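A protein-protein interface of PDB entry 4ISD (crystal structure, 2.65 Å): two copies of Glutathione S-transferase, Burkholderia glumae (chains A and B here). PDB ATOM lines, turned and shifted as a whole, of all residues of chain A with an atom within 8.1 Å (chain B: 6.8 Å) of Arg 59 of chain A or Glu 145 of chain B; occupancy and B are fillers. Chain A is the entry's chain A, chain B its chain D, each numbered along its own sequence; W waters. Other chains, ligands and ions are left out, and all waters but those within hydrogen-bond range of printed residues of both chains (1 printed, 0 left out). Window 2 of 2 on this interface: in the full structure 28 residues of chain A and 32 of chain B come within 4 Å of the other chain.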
ATOM      1  N   VAL A  40     -11.529 -12.660 -11.627  1.00  0.00           N
ATOM      2  CA  VAL A  40     -10.756 -11.620 -10.955  1.00  0.00           C
ATOM      3  C   VAL A  40     -10.867 -10.314 -11.764  1.00  0.00           C
ATOM      4  O   VAL A  40     -10.636 -10.310 -12.969  1.00  0.00           O
ATOM      5  CB  VAL A  40      -9.281 -12.054 -10.792  1.00  0.00           C
ATOM      6  CG1 VAL A  40      -8.562 -11.144  -9.823  1.00  0.00           C
ATOM      7  CG2 VAL A  40      -9.201 -13.501 -10.299  1.00  0.00           C
ATOM      8  N   SER A  44      -8.620  -3.536  -9.272  1.00  0.00           N
ATOM      9  CA  SER A  44      -7.243  -4.023  -9.407  1.00  0.00           C
ATOM     10  C   SER A  44      -7.098  -5.275  -8.534  1.00  0.00           C
ATOM     11  O   SER A  44      -6.073  -5.475  -7.863  1.00  0.00           O
ATOM     12  CB  SER A  44      -6.218  -2.964  -8.958  1.00  0.00           C
ATOM     13  OG  SER A  44      -5.281  -2.671  -9.989  1.00  0.00           O
ATOM     14  N   LYS A  45      -8.134  -6.114  -8.574  1.00  0.00           N
ATOM     15  CA  LYS A  45      -8.335  -7.222  -7.631  1.00  0.00           C
ATOM     16  C   LYS A  45      -7.237  -8.298  -7.538  1.00  0.00           C
ATOM     17  O   LYS A  45      -7.193  -9.044  -6.556  1.00  0.00           O
ATOM     18  CB  LYS A  45      -9.699  -7.885  -7.871  1.00  0.00           C
ATOM     19  N   GLN A  46      -6.345  -8.384  -8.522  1.00  0.00           N
ATOM     20  CA  GLN A  46      -5.261  -9.365  -8.445  1.00  0.00           C
ATOM     21  C   GLN A  46      -4.264  -9.017  -7.323  1.00  0.00           C
ATOM     22  O   GLN A  46      -3.184  -9.614  -7.222  1.00  0.00           O
ATOM     23  CB  GLN A  46      -4.532  -9.517  -9.791  1.00  0.00           C
ATOM     24  CG  GLN A  46      -3.714  -8.288 -10.234  1.00  0.00           C
ATOM     25  CD  GLN A  46      -4.537  -7.293 -11.060  1.00  0.00           C
ATOM     26  OE1 GLN A  46      -5.758  -7.156 -10.880  1.00  0.00           O
ATOM     27  NE2 GLN A  46      -3.869  -6.605 -11.983  1.00  0.00           N
ATOM     28  N   GLN A  47      -4.639  -8.066  -6.473  1.00  0.00           N
ATOM     29  CA  GLN A  47      -3.795  -7.640  -5.366  1.00  0.00           C
ATOM     30  C   GLN A  47      -4.607  -7.369  -4.082  1.00  0.00           C
ATOM     31  O   GLN A  47      -5.286  -8.261  -3.528  1.00  0.00           O
ATOM     32  CB  GLN A  47      -2.971  -6.421  -5.801  1.00  0.00           C
ATOM     33  CG  GLN A  47      -1.766  -6.793  -6.687  1.00  0.00           C
ATOM     34  CD  GLN A  47      -1.746  -6.131  -8.058  1.00  0.00           C
ATOM     35  OE1 GLN A  47      -2.644  -5.371  -8.403  1.00  0.00           O
ATOM     36  NE2 GLN A  47      -0.710  -6.425  -8.848  1.00  0.00           N
ATOM     37  N   GLU A  54      -2.545 -14.778  -2.250  1.00  0.00           N
ATOM     38  CA  GLU A  54      -3.646 -15.593  -1.717  1.00  0.00           C
ATOM     39  C   GLU A  54      -3.887 -16.950  -2.431  1.00  0.00           C
ATOM     40  O   GLU A  54      -3.717 -18.004  -1.823  1.00  0.00           O
ATOM     41  CB  GLU A  54      -4.936 -14.774  -1.636  1.00  0.00           C
ATOM     42  N   VAL A  55      -4.301 -16.947  -3.696  1.00  0.00           N
ATOM     43  CA  VAL A  55      -4.371 -18.218  -4.419  1.00  0.00           C
ATOM     44  C   VAL A  55      -3.318 -18.233  -5.498  1.00  0.00           C
ATOM     45  O   VAL A  55      -3.160 -19.236  -6.203  1.00  0.00           O
ATOM     46  CB  VAL A  55      -5.763 -18.541  -5.083  1.00  0.00           C
ATOM     47  CG1 VAL A  55      -6.856 -18.722  -4.045  1.00  0.00           C
ATOM     48  CG2 VAL A  55      -6.155 -17.496  -6.118  1.00  0.00           C
ATOM     49  N   SER A  56      -2.604 -17.117  -5.629  1.00  0.00           N
ATOM     50  CA  SER A  56      -1.683 -16.953  -6.745  1.00  0.00           C
ATOM     51  C   SER A  56      -0.397 -16.242  -6.398  1.00  0.00           C
ATOM     52  O   SER A  56      -0.391 -15.052  -6.096  1.00  0.00           O
ATOM     53  CB  SER A  56      -2.351 -16.188  -7.882  1.00  0.00           C
ATOM     54  OG  SER A  56      -1.396 -15.936  -8.898  1.00  0.00           O
ATOM     55  N   LEU A  57       0.704 -16.973  -6.485  1.00  0.00           N
ATOM     56  CA  LEU A  57       2.030 -16.422  -6.233  1.00  0.00           C
ATOM     57  C   LEU A  57       2.376 -15.253  -7.175  1.00  0.00           C
ATOM     58  O   LEU A  57       3.007 -14.292  -6.762  1.00  0.00           O
ATOM     59  CB  LEU A  57       3.075 -17.532  -6.364  1.00  0.00           C
ATOM     60  CG  LEU A  57       4.523 -17.075  -6.254  1.00  0.00           C
ATOM     61  CD1 LEU A  57       4.809 -16.632  -4.832  1.00  0.00           C
ATOM     62  CD2 LEU A  57       5.468 -18.185  -6.720  1.00  0.00           C
ATOM     63  N   THR A  58       1.950 -15.332  -8.430  1.00  0.00           N
ATOM     64  CA  THR A  58       2.336 -14.343  -9.437  1.00  0.00           C
ATOM     65  C   THR A  58       1.386 -13.148  -9.543  1.00  0.00           C
ATOM     66  O   THR A  58       1.729 -12.128 -10.148  1.00  0.00           O
ATOM     67  CB  THR A  58       2.374 -14.989 -10.813  1.00  0.00           C
ATOM     68  OG1 THR A  58       1.035 -15.333 -11.208  1.00  0.00           O
ATOM     69  CG2 THR A  58       3.214 -16.239 -10.771  1.00  0.00           C
ATOM     70  N   ARG A  59       0.191 -13.290  -8.974  1.00  0.00           N
ATOM     71  CA  ARG A  59      -0.868 -12.285  -9.082  1.00  0.00           C
ATOM     72  C   ARG A  59      -1.253 -11.996 -10.531  1.00  0.00           C
ATOM     73  O   ARG A  59      -1.497 -10.850 -10.910  1.00  0.00           O
ATOM     74  CB  ARG A  59      -0.489 -10.993  -8.372  1.00  0.00           C
ATOM     75  CG  ARG A  59      -0.150 -11.167  -6.894  1.00  0.00           C
ATOM     76  CD  ARG A  59      -0.060  -9.808  -6.237  1.00  0.00           C
ATOM     77  NE  ARG A  59       1.135  -9.652  -5.428  1.00  0.00           N
ATOM     78  CZ  ARG A  59       1.610  -8.478  -5.026  1.00  0.00           C
ATOM     79  NH1 ARG A  59       0.997  -7.356  -5.378  1.00  0.00           N
ATOM     80  NH2 ARG A  59       2.704  -8.425  -4.280  1.00  0.00           N
ATOM     81  N   ARG A  60      -1.294 -13.046 -11.339  1.00  0.00           N
ATOM     82  CA  ARG A  60      -1.831 -12.946 -12.679  1.00  0.00           C
ATOM     83  C   ARG A  60      -2.844 -14.070 -12.927  1.00  0.00           C
ATOM     84  O   ARG A  60      -2.811 -15.120 -12.269  1.00  0.00           O
ATOM     85  CB  ARG A  60      -0.700 -12.984 -13.700  1.00  0.00           C
ATOM     86  CG  ARG A  60       0.343 -11.895 -13.470  1.00  0.00           C
ATOM     87  CD  ARG A  60       1.195 -11.670 -14.710  1.00  0.00           C
ATOM     88  NE  ARG A  60       1.961 -12.863 -15.061  1.00  0.00           N
ATOM     89  CZ  ARG A  60       2.897 -12.881 -16.002  1.00  0.00           C
ATOM     90  NH1 ARG A  60       3.572 -14.001 -16.267  1.00  0.00           N
ATOM     91  NH2 ARG A  60       3.163 -11.765 -16.670  1.00  0.00           N
ATOM     92  N   VAL A  61      -3.775 -13.829 -13.845  1.00  0.00           N
ATOM     93  CA  VAL A  61      -4.686 -14.873 -14.281  1.00  0.00           C
ATOM     94  C   VAL A  61      -4.073 -15.470 -15.540  1.00  0.00           C
ATOM     95  O   VAL A  61      -3.372 -14.771 -16.273  1.00  0.00           O
ATOM     96  CB  VAL A  61      -6.095 -14.314 -14.580  1.00  0.00           C
ATOM     97  CG1 VAL A  61      -6.808 -13.909 -13.290  1.00  0.00           C
ATOM     98  CG2 VAL A  61      -6.011 -13.131 -15.540  1.00  0.00           C
ATOM     99  N   PRO A  62      -4.300 -16.768 -15.794  1.00  0.00           N
ATOM    100  CA  PRO A  62      -5.060 -17.747 -15.006  1.00  0.00           C
ATOM    101  C   PRO A  62      -4.315 -18.321 -13.793  1.00  0.00           C
ATOM    102  O   PRO A  62      -3.083 -18.301 -13.709  1.00  0.00           O
ATOM    103  CB  PRO A  62      -5.281 -18.873 -16.014  1.00  0.00           C
ATOM    104  CG  PRO A  62      -4.005 -18.831 -16.824  1.00  0.00           C
ATOM    105  CD  PRO A  62      -3.789 -17.363 -17.041  1.00  0.00           C
ATOM    106  N   THR A  63      -5.095 -18.840 -12.853  1.00  0.00           N
ATOM    107  CA  THR A  63      -4.582 -19.666 -11.775  1.00  0.00           C
ATOM    108  C   THR A  63      -5.490 -20.886 -11.651  1.00  0.00           C
ATOM    109  O   THR A  63      -6.715 -20.766 -11.731  1.00  0.00           O
ATOM    110  CB  THR A  63      -4.593 -18.908 -10.451  1.00  0.00           C
ATOM    111  OG1 THR A  63      -3.703 -17.786 -10.537  1.00  0.00           O
ATOM    112  CG2 THR A  63      -4.171 -19.827  -9.306  1.00  0.00           C
ATOM    113  N   SER A  72      -0.307 -21.179 -10.899  1.00  0.00           N
ATOM    114  CA  SER A  72      -0.438 -20.142 -11.941  1.00  0.00           C
ATOM    115  C   SER A  72       0.414 -20.450 -13.185  1.00  0.00           C
ATOM    116  O   SER A  72       1.025 -21.516 -13.264  1.00  0.00           O
ATOM    117  CB  SER A  72      -0.106 -18.758 -11.382  1.00  0.00           C
ATOM    118  OG  SER A  72      -1.232 -18.193 -10.714  1.00  0.00           O
ATOM    119  N   GLU A  73       0.444 -19.525 -14.148  1.00  0.00           N
ATOM    120  CA  GLU A  73       1.147 -19.724 -15.427  1.00  0.00           C
ATOM    121  C   GLU A  73       0.505 -20.840 -16.261  1.00  0.00           C
ATOM    122  O   GLU A  73       0.673 -22.042 -15.966  1.00  0.00           O
ATOM    123  CB  GLU A  73       2.649 -19.985 -15.250  1.00  0.00           C
ATOM    124  CG  GLU A  73       3.424 -18.830 -14.629  1.00  0.00           C
ATOM    125  CD  GLU A  73       3.486 -17.625 -15.547  1.00  0.00           C
ATOM    126  OE1 GLU A  73       3.883 -17.819 -16.713  1.00  0.00           O
ATOM    127  OE2 GLU A  73       3.123 -16.499 -15.110  1.00  0.00           O
ATOM    128  N   TRP B 110       7.182 -17.806 -14.981  1.00  0.00           N
ATOM    129  CA  TRP B 110       6.912 -16.489 -14.400  1.00  0.00           C
ATOM    130  C   TRP B 110       8.094 -15.581 -14.678  1.00  0.00           C
ATOM    131  O   TRP B 110       7.939 -14.476 -15.213  1.00  0.00           O
ATOM    132  CB  TRP B 110       6.672 -16.589 -12.906  1.00  0.00           C
ATOM    133  CG  TRP B 110       6.209 -15.313 -12.271  1.00  0.00           C
ATOM    134  CD1 TRP B 110       5.546 -14.284 -12.874  1.00  0.00           C
ATOM    135  CD2 TRP B 110       6.377 -14.936 -10.900  1.00  0.00           C
ATOM    136  NE1 TRP B 110       5.292 -13.288 -11.961  1.00  0.00           N
ATOM    137  CE2 TRP B 110       5.789 -13.667 -10.740  1.00  0.00           C
ATOM    138  CE3 TRP B 110       6.953 -15.557  -9.789  1.00  0.00           C
ATOM    139  CZ2 TRP B 110       5.769 -13.002  -9.514  1.00  0.00           C
ATOM    140  CZ3 TRP B 110       6.942 -14.894  -8.574  1.00  0.00           C
ATOM    141  CH2 TRP B 110       6.357 -13.629  -8.446  1.00  0.00           C
ATOM    142  N   ASP B 114       7.498 -12.059 -16.840  1.00  0.00           N
ATOM    143  CA  ASP B 114       7.034 -10.955 -16.008  1.00  0.00           C
ATOM    144  C   ASP B 114       8.224 -10.087 -15.608  1.00  0.00           C
ATOM    145  O   ASP B 114       9.307 -10.247 -16.178  1.00  0.00           O
ATOM    146  CB  ASP B 114       6.286 -11.476 -14.784  1.00  0.00           C
ATOM    147  CG  ASP B 114       5.323 -10.453 -14.213  1.00  0.00           C
ATOM    148  OD1 ASP B 114       5.397  -9.274 -14.627  1.00  0.00           O
ATOM    149  OD2 ASP B 114       4.500 -10.830 -13.347  1.00  0.00           O
ATOM    150  N   LEU B 118      11.822  -4.108 -14.773  1.00  0.00           N
ATOM    151  CA  LEU B 118      13.129  -4.152 -14.116  1.00  0.00           C
ATOM    152  C   LEU B 118      14.275  -4.515 -15.063  1.00  0.00           C
ATOM    153  O   LEU B 118      14.048  -4.964 -16.191  1.00  0.00           O
ATOM    154  CB  LEU B 118      13.096  -5.115 -12.926  1.00  0.00           C
ATOM    155  CG  LEU B 118      12.052  -4.813 -11.844  1.00  0.00           C
ATOM    156  CD1 LEU B 118      12.101  -5.852 -10.737  1.00  0.00           C
ATOM    157  CD2 LEU B 118      12.241  -3.408 -11.284  1.00  0.00           C
ATOM    158  N   ALA B 140       7.417  -0.411 -12.019  1.00  0.00           N
ATOM    159  CA  ALA B 140       8.650  -0.996 -11.491  1.00  0.00           C
ATOM    160  C   ALA B 140       8.486  -1.362 -10.020  1.00  0.00           C
ATOM    161  O   ALA B 140       8.829  -2.477  -9.614  1.00  0.00           O
ATOM    162  CB  ALA B 140       9.840  -0.063 -11.689  1.00  0.00           C
ATOM    163  N   GLN B 141       7.928  -0.434  -9.244  1.00  0.00           N
ATOM    164  CA  GLN B 141       7.654  -0.659  -7.832  1.00  0.00           C
ATOM    165  C   GLN B 141       6.799  -1.915  -7.612  1.00  0.00           C
ATOM    166  O   GLN B 141       6.978  -2.640  -6.618  1.00  0.00           O
ATOM    167  CB  GLN B 141       6.962   0.564  -7.239  1.00  0.00           C
ATOM    168  CG  GLN B 141       6.718   0.492  -5.742  1.00  0.00           C
ATOM    169  CD  GLN B 141       6.326   1.841  -5.169  1.00  0.00           C
ATOM    170  OE1 GLN B 141       6.869   2.876  -5.564  1.00  0.00           O
ATOM    171  NE2 GLN B 141       5.376   1.840  -4.240  1.00  0.00           N
ATOM    172  N   LEU B 142       5.893  -2.185  -8.549  1.00  0.00           N
ATOM    173  CA  LEU B 142       5.004  -3.337  -8.423  1.00  0.00           C
ATOM    174  C   LEU B 142       5.725  -4.661  -8.692  1.00  0.00           C
ATOM    175  O   LEU B 142       5.476  -5.659  -8.016  1.00  0.00           O
ATOM    176  CB  LEU B 142       3.808  -3.187  -9.353  1.00  0.00           C
ATOM    177  CG  LEU B 142       2.716  -4.247  -9.245  1.00  0.00           C
ATOM    178  CD1 LEU B 142       1.543  -3.756  -8.392  1.00  0.00           C
ATOM    179  CD2 LEU B 142       2.256  -4.699 -10.641  1.00  0.00           C
ATOM    180  N   ALA B 143       6.602  -4.673  -9.688  1.00  0.00           N
ATOM    181  CA  ALA B 143       7.396  -5.860  -9.980  1.00  0.00           C
ATOM    182  C   ALA B 143       8.257  -6.209  -8.772  1.00  0.00           C
ATOM    183  O   ALA B 143       8.276  -7.356  -8.313  1.00  0.00           O
ATOM    184  CB  ALA B 143       8.275  -5.631 -11.194  1.00  0.00           C
ATOM    185  N   CYS B 144       8.976  -5.204  -8.282  1.00  0.00           N
ATOM    186  CA  CYS B 144       9.778  -5.330  -7.075  1.00  0.00           C
ATOM    187  C   CYS B 144       8.975  -5.968  -5.956  1.00  0.00           C
ATOM    188  O   CYS B 144       9.423  -6.927  -5.323  1.00  0.00           O
ATOM    189  CB  CYS B 144      10.264  -3.956  -6.623  1.00  0.00           C
ATOM    190  SG  CYS B 144      11.511  -3.263  -7.721  1.00  0.00           S
ATOM    191  N   GLU B 145       7.773  -5.443  -5.744  1.00  0.00           N
ATOM    192  CA  GLU B 145       6.942  -5.869  -4.634  1.00  0.00           C
ATOM    193  C   GLU B 145       6.509  -7.330  -4.795  1.00  0.00           C
ATOM    194  O   GLU B 145       6.292  -8.033  -3.806  1.00  0.00           O
ATOM    195  CB  GLU B 145       5.744  -4.931  -4.483  1.00  0.00           C
ATOM    196  CG  GLU B 145       4.964  -5.117  -3.208  1.00  0.00           C
ATOM    197  CD  GLU B 145       3.478  -4.809  -3.381  1.00  0.00           C
ATOM    198  OE1 GLU B 145       3.140  -3.825  -4.084  1.00  0.00           O
ATOM    199  OE2 GLU B 145       2.650  -5.558  -2.813  1.00  0.00           O
ATOM    200  N   LYS B 146       6.409  -7.790  -6.039  1.00  0.00           N
ATOM    201  CA  LYS B 146       6.014  -9.174  -6.314  1.00  0.00           C
ATOM    202  C   LYS B 146       7.222 -10.091  -6.182  1.00  0.00           C
ATOM    203  O   LYS B 146       7.131 -11.191  -5.634  1.00  0.00           O
ATOM    204  CB  LYS B 146       5.389  -9.318  -7.717  1.00  0.00           C
ATOM    205  CG  LYS B 146       3.964  -8.793  -7.818  1.00  0.00           C
ATOM    206  CD  LYS B 146       3.206  -9.387  -9.000  1.00  0.00           C
ATOM    207  CE  LYS B 146       3.840  -9.044 -10.339  1.00  0.00           C
ATOM    208  NZ  LYS B 146       3.101  -9.712 -11.459  1.00  0.00           N
ATOM    209  N   LEU B 147       8.351  -9.627  -6.698  1.00  0.00           N
ATOM    210  CA  LEU B 147       9.596 -10.369  -6.606  1.00  0.00           C
ATOM    211  C   LEU B 147      10.048 -10.515  -5.140  1.00  0.00           C
ATOM    212  O   LEU B 147      10.407 -11.601  -4.680  1.00  0.00           O
ATOM    213  CB  LEU B 147      10.667  -9.649  -7.392  1.00  0.00           C
ATOM    214  CG  LEU B 147      11.965 -10.433  -7.386  1.00  0.00           C
ATOM    215  CD1 LEU B 147      11.722 -11.807  -7.996  1.00  0.00           C
ATOM    216  CD2 LEU B 147      13.036  -9.647  -8.138  1.00  0.00           C
ATOM    217  N   LEU B 148      10.015  -9.416  -4.401  1.00  0.00           N
ATOM    218  CA  LEU B 148      10.355  -9.492  -3.005  1.00  0.00           C
ATOM    219  C   LEU B 148       9.397 -10.439  -2.302  1.00  0.00           C
ATOM    220  O   LEU B 148       9.834 -11.342  -1.572  1.00  0.00           O
ATOM    221  CB  LEU B 148      10.370  -8.111  -2.346  1.00  0.00           C
ATOM    222  CG  LEU B 148      10.827  -8.172  -0.890  1.00  0.00           C
ATOM    223  CD1 LEU B 148      12.036  -9.109  -0.764  1.00  0.00           C
ATOM    224  CD2 LEU B 148      11.135  -6.765  -0.349  1.00  0.00           C
ATOM    225  N   SER B 149       8.101 -10.264  -2.545  1.00  0.00           N
ATOM    226  CA  SER B 149       7.107 -11.037  -1.805  1.00  0.00           C
ATOM    227  C   SER B 149       7.319 -12.521  -2.042  1.00  0.00           C
ATOM    228  O   SER B 149       7.198 -13.323  -1.123  1.00  0.00           O
ATOM    229  CB  SER B 149       5.690 -10.618  -2.175  1.00  0.00           C
ATOM    230  OG  SER B 149       4.779 -10.980  -1.153  1.00  0.00           O
ATOM    231  N   ALA B 150       7.687 -12.872  -3.271  1.00  0.00           N
ATOM    232  CA  ALA B 150       7.918 -14.271  -3.632  1.00  0.00           C
ATOM    233  C   ALA B 150       9.193 -14.824  -2.981  1.00  0.00           C
ATOM    234  O   ALA B 150       9.180 -15.942  -2.449  1.00  0.00           O
ATOM    235  CB  ALA B 150       7.970 -14.440  -5.153  1.00  0.00           C
ATOM    236  N   LEU B 180      16.668  -7.065  -7.025  1.00  0.00           N
ATOM    237  CA  LEU B 180      16.179  -6.465  -5.794  1.00  0.00           C
ATOM    238  C   LEU B 180      17.088  -5.305  -5.392  1.00  0.00           C
ATOM    239  O   LEU B 180      16.656  -4.381  -4.706  1.00  0.00           O
ATOM    240  CB  LEU B 180      16.092  -7.502  -4.678  1.00  0.00           C
ATOM    241  CG  LEU B 180      14.979  -8.535  -4.878  1.00  0.00           C
ATOM    242  CD1 LEU B 180      14.964  -9.500  -3.714  1.00  0.00           C
ATOM    243  CD2 LEU B 180      13.643  -7.845  -5.021  1.00  0.00           C
ATOM    244  N   CYS B 183      15.588  -2.116  -6.328  1.00  0.00           N
ATOM    245  CA  CYS B 183      14.308  -1.767  -5.725  1.00  0.00           C
ATOM    246  C   CYS B 183      14.502  -0.921  -4.453  1.00  0.00           C
ATOM    247  O   CYS B 183      15.593  -0.375  -4.205  1.00  0.00           O
ATOM    248  CB  CYS B 183      13.460  -3.014  -5.474  1.00  0.00           C
ATOM    249  SG  CYS B 183      13.219  -4.082  -6.961  1.00  0.00           S
ATOM    250  N   ASP B 185      12.662  -1.595  -1.165  1.00  0.00           N
ATOM    251  CA  ASP B 185      12.284  -2.209   0.108  1.00  0.00           C
ATOM    252  C   ASP B 185      13.320  -3.192   0.682  1.00  0.00           C
ATOM    253  O   ASP B 185      13.961  -3.945  -0.055  1.00  0.00           O
ATOM    254  CB  ASP B 185      10.903  -2.848   0.005  1.00  0.00           C
ATOM    255  CG  ASP B 185       9.785  -1.836   0.197  1.00  0.00           C
ATOM    256  OD1 ASP B 185       9.475  -1.521   1.371  1.00  0.00           O
ATOM    257  OD2 ASP B 185       9.222  -1.354  -0.812  1.00  0.00           O
HETATM  258  O   HOH W   1       0.366  -8.650 -11.399  1.00  0.00           O
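The guanidinium group (NE) of Arg 60 of chain A is in salt-bridge range of the side-chain carboxylate (OD2) of Asp 114 of chain B, 3.7 Å away.
The side-chain carboxylate (OE2) of Glu 145 of chain B lies within salt-bridge range of the guanidinium group (NH2) of Arg 59 of chain A (3.2 Å).
O of Thr 58 of chain A lies within hydrogen-bond range of NZ of Lys 146 of chain B (3.1 Å).
The side-chain carboxylate (OD2) of Asp 114 of chain B lies within salt-bridge range of the side-chain amino group (NZ) of Lys 146 of chain B, at 2.6 Å.
The side-chain hydroxyl of Thr 63 of chain A lies within hydrogen-bond range of the backbone carbonyl oxygen of Arg 60 of chain A (3.3 Å).
OE2 of Glu 73 of chain A lies within salt-bridge range of NH1 of Arg 60 of chain A, 2.8 Å away.
The backbone carbonyl oxygen of Ser 44 of chain A lies close to the side-chain amide oxygen of Gln 47 of chain A (3.5 Å).
The side-chain hydroxyl of Thr 58 of chain A lies close to the backbone NH of Arg 60 of chain A, 3.3 Å away.
The indole nitrogen (NE1) of Trp 110 of chain B sits at hydrogen-bond distance from the side-chain carboxylate (OD2) of Asp 114 of chain B (2.9 Å).
Among the printed residues, merely in contact across the chains: Thr 58 of chain A with Trp 110 of chain B, Gln 47 of chain A with Leu 142 of chain B, Arg 59 of chain A with Lys 146 of chain B, Glu 73 of chain A with Trp 110 of chain B, Leu 57 of chain A with Trp 110 of chain B, Leu 57 of chain A with Ala 150 of chain B and Arg 60 of chain A with Trp 110 of chain B.
Arg 59 of chain A touches just these residues of chain B: Glu 145 and Lys 146.
Glu 145 of chain B touches just one residue of chain A: Arg 59.
Of the printed residues of chain A, Leu 142 of chain B touches Gln 47 (3.5 Å).
Of the printed residues of chain A, Ala 150 of chain B touches Leu 57.
The nearest residue of chain B that does not touch Arg 59 of chain A is Ser 149 of chain B (4.3 Å).
The nearest residue of chain A that does not touch Glu 145 of chain B is Gln 47 of chain A (6.0 Å).
The nearest printed residue of chain A that does not touch Ala 150 of chain B is Arg 59 of chain A (6.8 Å).
Of the 17 printed residues of chain B, 6 touch a printed residue of chain A.
Printed residues of chain B that touch a printed residue of chain A: Trp 110, Asp 114, Leu 142, Glu 145, Lys 146 and Ala 150.
Hydrophobic or aromatic side chains of chain B within 4 Å of the printed part of chain A: Trp 110, Leu 142 and Ala 150.
Hydrophobic or aromatic side chains of chain A that line the printed part of chain B: Leu 57.
Among the printed residues, Asp or Glu carboxylates within 4 Å of a Lys or Arg side-chain nitrogen of the other chain: Arg 59 of chain A with Glu 145 of chain B (3.2 Å) and Arg 60 of chain A with Asp 114 of chain B (3.7 Å).
No position is printed for both chains.
Of the 10 pairs that touch across the chains among the printed residues, none has its exchanged pair printed and touching as well.
Water W1 bridges the backbone carbonyl oxygen (O) of Arg 59 of chain A (2.9 Å) and the side-chain amino group (NZ) of Lys 146 of chain B (2.9 Å).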
